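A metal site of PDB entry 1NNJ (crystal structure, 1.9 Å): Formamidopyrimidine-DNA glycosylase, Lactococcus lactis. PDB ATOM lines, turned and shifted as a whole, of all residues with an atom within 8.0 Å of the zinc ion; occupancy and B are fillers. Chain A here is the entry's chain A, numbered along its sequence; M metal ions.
The side-chain sulfur (SG) of Cys 268 sits close to the guanidinium group (NE) of Arg 247 (3.5 Å). SG of Cys 245 lies close to NE1 of Trp 179 (3.4 Å). N of Arg 247 sits close to SG of Cys 245 (3.3 Å). The backbone carbonyl oxygen (O) of Ala 250 is in hydrogen-bond range of the backbone NH (N) of Cys 245 (2.6 Å). The side-chain sulfur (SG) of Cys 248 lies close to the backbone NH (N) of Ala 250, at 3.3 Å. SG of Cys 265 sits close to N of Val 267 (3.5 Å). The backbone NH (N) of Cys 265 lies within hydrogen-bond range of the side-chain amide oxygen (OE1) of Gln 269, at 3.0 Å.
Of the 18 residues printed, 4 come within 4 Å of the zinc ion. The nearest printed residue that does not touch the zinc ion is Val 267 (4.3 Å).
The zinc ion is bound by the side-chain sulfur (SG) of Cys 265, the side-chain sulfur (SG) of Cys 245, the side-chain sulfur (SG) of Cys 268 and the side-chain sulfur (SG) of Cys 248.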
ATOM      1  N   TRP A 179      25.612 -18.304   2.380  1.00  0.00           N
ATOM      2  CA  TRP A 179      26.065 -19.511   1.702  1.00  0.00           C
ATOM      3  C   TRP A 179      27.360 -19.187   0.949  1.00  0.00           C
ATOM      4  O   TRP A 179      28.289 -19.983   0.913  1.00  0.00           O
ATOM      5  CB  TRP A 179      25.023 -20.010   0.699  1.00  0.00           C
ATOM      6  CG  TRP A 179      25.489 -21.189  -0.137  1.00  0.00           C
ATOM      7  CD1 TRP A 179      25.397 -22.523   0.184  1.00  0.00           C
ATOM      8  CD2 TRP A 179      26.144 -21.133  -1.419  1.00  0.00           C
ATOM      9  NE1 TRP A 179      25.946 -23.291  -0.820  1.00  0.00           N
ATOM     10  CE2 TRP A 179      26.411 -22.459  -1.809  1.00  0.00           C
ATOM     11  CE3 TRP A 179      26.521 -20.081  -2.268  1.00  0.00           C
ATOM     12  CZ2 TRP A 179      27.047 -22.771  -3.025  1.00  0.00           C
ATOM     13  CZ3 TRP A 179      27.151 -20.390  -3.472  1.00  0.00           C
ATOM     14  CH2 TRP A 179      27.408 -21.721  -3.833  1.00  0.00           C
ATOM     15  N   LYS A 182      30.158 -18.968   3.386  1.00  0.00           N
ATOM     16  CA  LYS A 182      30.288 -20.180   4.182  1.00  0.00           C
ATOM     17  C   LYS A 182      30.107 -19.964   5.686  1.00  0.00           C
ATOM     18  O   LYS A 182      30.905 -20.433   6.501  1.00  0.00           O
ATOM     19  CB  LYS A 182      31.649 -20.836   3.905  1.00  0.00           C
ATOM     20  CG  LYS A 182      31.860 -21.186   2.437  1.00  0.00           C
ATOM     21  CD  LYS A 182      33.199 -21.856   2.195  1.00  0.00           C
ATOM     22  CE  LYS A 182      33.389 -22.161   0.712  1.00  0.00           C
ATOM     23  NZ  LYS A 182      34.661 -22.906   0.447  1.00  0.00           N
ATOM     24  N   VAL A 237      20.806 -21.131  -2.850  1.00  0.00           N
ATOM     25  CA  VAL A 237      20.125 -21.800  -1.748  1.00  0.00           C
ATOM     26  C   VAL A 237      18.684 -21.397  -1.460  1.00  0.00           C
ATOM     27  O   VAL A 237      17.882 -22.244  -1.053  1.00  0.00           O
ATOM     28  CB  VAL A 237      20.927 -21.645  -0.422  1.00  0.00           C
ATOM     29  CG1 VAL A 237      22.207 -22.443  -0.504  1.00  0.00           C
ATOM     30  CG2 VAL A 237      21.225 -20.170  -0.165  1.00  0.00           C
ATOM     31  N   LYS A 244      20.738 -30.261  -4.518  1.00  0.00           N
ATOM     32  CA  LYS A 244      22.152 -30.419  -4.190  1.00  0.00           C
ATOM     33  C   LYS A 244      22.929 -29.121  -4.251  1.00  0.00           C
ATOM     34  O   LYS A 244      22.777 -28.322  -5.182  1.00  0.00           O
ATOM     35  CB  LYS A 244      22.809 -31.410  -5.167  1.00  0.00           C
ATOM     36  CG  LYS A 244      21.938 -32.571  -5.603  1.00  0.00           C
ATOM     37  CD  LYS A 244      21.485 -33.428  -4.437  1.00  0.00           C
ATOM     38  CE  LYS A 244      20.595 -34.561  -4.932  1.00  0.00           C
ATOM     39  NZ  LYS A 244      20.080 -35.402  -3.819  1.00  0.00           N
ATOM     40  N   CYS A 245      23.776 -28.899  -3.240  1.00  0.00           N
ATOM     41  CA  CYS A 245      24.610 -27.704  -3.194  1.00  0.00           C
ATOM     42  C   CYS A 245      25.529 -27.750  -4.402  1.00  0.00           C
ATOM     43  O   CYS A 245      26.071 -28.809  -4.738  1.00  0.00           O
ATOM     44  CB  CYS A 245      25.430 -27.696  -1.900  1.00  0.00           C
ATOM     45  SG  CYS A 245      26.726 -26.452  -1.856  1.00  0.00           S
ATOM     46  N   SER A 246      25.704 -26.610  -5.060  1.00  0.00           N
ATOM     47  CA  SER A 246      26.547 -26.542  -6.257  1.00  0.00           C
ATOM     48  C   SER A 246      28.050 -26.670  -5.973  1.00  0.00           C
ATOM     49  O   SER A 246      28.838 -26.808  -6.912  1.00  0.00           O
ATOM     50  CB  SER A 246      26.286 -25.238  -7.007  1.00  0.00           C
ATOM     51  OG  SER A 246      26.672 -24.120  -6.228  1.00  0.00           O
ATOM     52  N   ARG A 247      28.436 -26.620  -4.711  1.00  0.00           N
ATOM     53  CA  ARG A 247      29.862 -26.731  -4.366  1.00  0.00           C
ATOM     54  C   ARG A 247      30.267 -28.096  -3.827  1.00  0.00           C
ATOM     55  O   ARG A 247      31.261 -28.664  -4.270  1.00  0.00           O
ATOM     56  CB  ARG A 247      30.262 -25.671  -3.335  1.00  0.00           C
ATOM     57  CG  ARG A 247      30.427 -24.272  -3.906  1.00  0.00           C
ATOM     58  CD  ARG A 247      30.919 -23.303  -2.834  1.00  0.00           C
ATOM     59  NE  ARG A 247      30.061 -23.334  -1.655  1.00  0.00           N
ATOM     60  CZ  ARG A 247      29.817 -22.285  -0.865  1.00  0.00           C
ATOM     61  NH1 ARG A 247      30.377 -21.113  -1.144  1.00  0.00           N
ATOM     62  NH2 ARG A 247      29.018 -22.417   0.175  1.00  0.00           N
ATOM     63  N   CYS A 248      29.500 -28.622  -2.875  1.00  0.00           N
ATOM     64  CA  CYS A 248      29.848 -29.902  -2.267  1.00  0.00           C
ATOM     65  C   CYS A 248      28.930 -31.064  -2.621  1.00  0.00           C
ATOM     66  O   CYS A 248      29.316 -32.219  -2.438  1.00  0.00           O
ATOM     67  CB  CYS A 248      29.901 -29.750  -0.755  1.00  0.00           C
ATOM     68  SG  CYS A 248      28.287 -29.712   0.036  1.00  0.00           S
ATOM     69  N   GLY A 249      27.727 -30.764  -3.099  1.00  0.00           N
ATOM     70  CA  GLY A 249      26.804 -31.825  -3.467  1.00  0.00           C
ATOM     71  C   GLY A 249      25.814 -32.220  -2.388  1.00  0.00           C
ATOM     72  O   GLY A 249      24.912 -33.020  -2.636  1.00  0.00           O
ATOM     73  N   ALA A 250      25.970 -31.686  -1.174  1.00  0.00           N
ATOM     74  CA  ALA A 250      25.049 -32.023  -0.091  1.00  0.00           C
ATOM     75  C   ALA A 250      23.679 -31.378  -0.342  1.00  0.00           C
ATOM     76  O   ALA A 250      23.585 -30.395  -1.072  1.00  0.00           O
ATOM     77  CB  ALA A 250      25.607 -31.550   1.242  1.00  0.00           C
ATOM     78  N   GLU A 251      22.641 -31.936   0.257  1.00  0.00           N
ATOM     79  CA  GLU A 251      21.290 -31.393   0.094  1.00  0.00           C
ATOM     80  C   GLU A 251      21.057 -30.129   0.904  1.00  0.00           C
ATOM     81  O   GLU A 251      21.347 -30.074   2.098  1.00  0.00           O
ATOM     82  CB  GLU A 251      20.226 -32.415   0.504  1.00  0.00           C
ATOM     83  CG  GLU A 251      19.832 -33.387  -0.582  1.00  0.00           C
ATOM     84  CD  GLU A 251      18.499 -34.057  -0.294  1.00  0.00           C
ATOM     85  OE1 GLU A 251      18.111 -34.951  -1.086  1.00  0.00           O
ATOM     86  OE2 GLU A 251      17.839 -33.694   0.699  1.00  0.00           O
ATOM     87  N   ILE A 252      20.521 -29.106   0.245  1.00  0.00           N
ATOM     88  CA  ILE A 252      20.227 -27.845   0.909  1.00  0.00           C
ATOM     89  C   ILE A 252      19.086 -28.105   1.889  1.00  0.00           C
ATOM     90  O   ILE A 252      18.082 -28.727   1.530  1.00  0.00           O
ATOM     91  CB  ILE A 252      19.791 -26.768  -0.107  1.00  0.00           C
ATOM     92  CG1 ILE A 252      20.921 -26.517  -1.107  1.00  0.00           C
ATOM     93  CG2 ILE A 252      19.404 -25.490   0.627  1.00  0.00           C
ATOM     94  CD1 ILE A 252      22.258 -26.107  -0.484  1.00  0.00           C
ATOM     95  N   PHE A 264      20.145 -23.331   3.780  1.00  0.00           N
ATOM     96  CA  PHE A 264      21.602 -23.403   3.885  1.00  0.00           C
ATOM     97  C   PHE A 264      22.137 -24.801   3.565  1.00  0.00           C
ATOM     98  O   PHE A 264      21.391 -25.778   3.569  1.00  0.00           O
ATOM     99  CB  PHE A 264      22.026 -23.013   5.303  1.00  0.00           C
ATOM    100  CG  PHE A 264      21.725 -24.065   6.347  1.00  0.00           C
ATOM    101  CD1 PHE A 264      22.708 -24.946   6.782  1.00  0.00           C
ATOM    102  CD2 PHE A 264      20.440 -24.197   6.873  1.00  0.00           C
ATOM    103  CE1 PHE A 264      22.430 -25.939   7.724  1.00  0.00           C
ATOM    104  CE2 PHE A 264      20.145 -25.176   7.818  1.00  0.00           C
ATOM    105  CZ  PHE A 264      21.144 -26.058   8.245  1.00  0.00           C
ATOM    106  N   CYS A 265      23.444 -24.874   3.280  1.00  0.00           N
ATOM    107  CA  CYS A 265      24.104 -26.150   3.024  1.00  0.00           C
ATOM    108  C   CYS A 265      24.809 -26.520   4.321  1.00  0.00           C
ATOM    109  O   CYS A 265      25.682 -25.788   4.794  1.00  0.00           O
ATOM    110  CB  CYS A 265      25.133 -26.017   1.897  1.00  0.00           C
ATOM    111  SG  CYS A 265      26.234 -27.503   1.731  1.00  0.00           S
ATOM    112  N   PRO A 266      24.436 -27.658   4.934  1.00  0.00           N
ATOM    113  CA  PRO A 266      25.001 -28.167   6.188  1.00  0.00           C
ATOM    114  C   PRO A 266      26.501 -28.458   6.154  1.00  0.00           C
ATOM    115  O   PRO A 266      27.150 -28.534   7.194  1.00  0.00           O
ATOM    116  CB  PRO A 266      24.182 -29.433   6.457  1.00  0.00           C
ATOM    117  CG  PRO A 266      22.909 -29.197   5.713  1.00  0.00           C
ATOM    118  CD  PRO A 266      23.391 -28.571   4.445  1.00  0.00           C
ATOM    119  N   VAL A 267      27.041 -28.648   4.961  1.00  0.00           N
ATOM    120  CA  VAL A 267      28.466 -28.936   4.806  1.00  0.00           C
ATOM    121  C   VAL A 267      29.271 -27.647   4.688  1.00  0.00           C
ATOM    122  O   VAL A 267      30.222 -27.434   5.436  1.00  0.00           O
ATOM    123  CB  VAL A 267      28.736 -29.796   3.542  1.00  0.00           C
ATOM    124  CG1 VAL A 267      30.234 -29.925   3.306  1.00  0.00           C
ATOM    125  CG2 VAL A 267      28.107 -31.177   3.720  1.00  0.00           C
ATOM    126  N   CYS A 268      28.883 -26.790   3.757  1.00  0.00           N
ATOM    127  CA  CYS A 268      29.583 -25.535   3.512  1.00  0.00           C
ATOM    128  C   CYS A 268      29.401 -24.515   4.630  1.00  0.00           C
ATOM    129  O   CYS A 268      30.256 -23.644   4.826  1.00  0.00           O
ATOM    130  CB  CYS A 268      29.110 -24.932   2.181  1.00  0.00           C
ATOM    131  SG  CYS A 268      29.611 -25.844   0.683  1.00  0.00           S
ATOM    132  N   GLN A 269      28.300 -24.626   5.376  1.00  0.00           N
ATOM    133  CA  GLN A 269      28.012 -23.701   6.472  1.00  0.00           C
ATOM    134  C   GLN A 269      27.956 -24.459   7.802  1.00  0.00           C
ATOM    135  O   GLN A 269      26.875 -24.729   8.331  1.00  0.00           O
ATOM    136  CB  GLN A 269      26.691 -22.972   6.200  1.00  0.00           C
ATOM    137  CG  GLN A 269      26.750 -22.052   4.975  1.00  0.00           C
ATOM    138  CD  GLN A 269      25.376 -21.609   4.491  1.00  0.00           C
ATOM    139  OE1 GLN A 269      24.766 -22.242   3.619  1.00  0.00           O
ATOM    140  NE2 GLN A 269      24.873 -20.525   5.063  1.00  0.00           N
HETATM  141 ZN    ZN M   1      27.742 -27.286   0.166  1.00  0.00          ZN
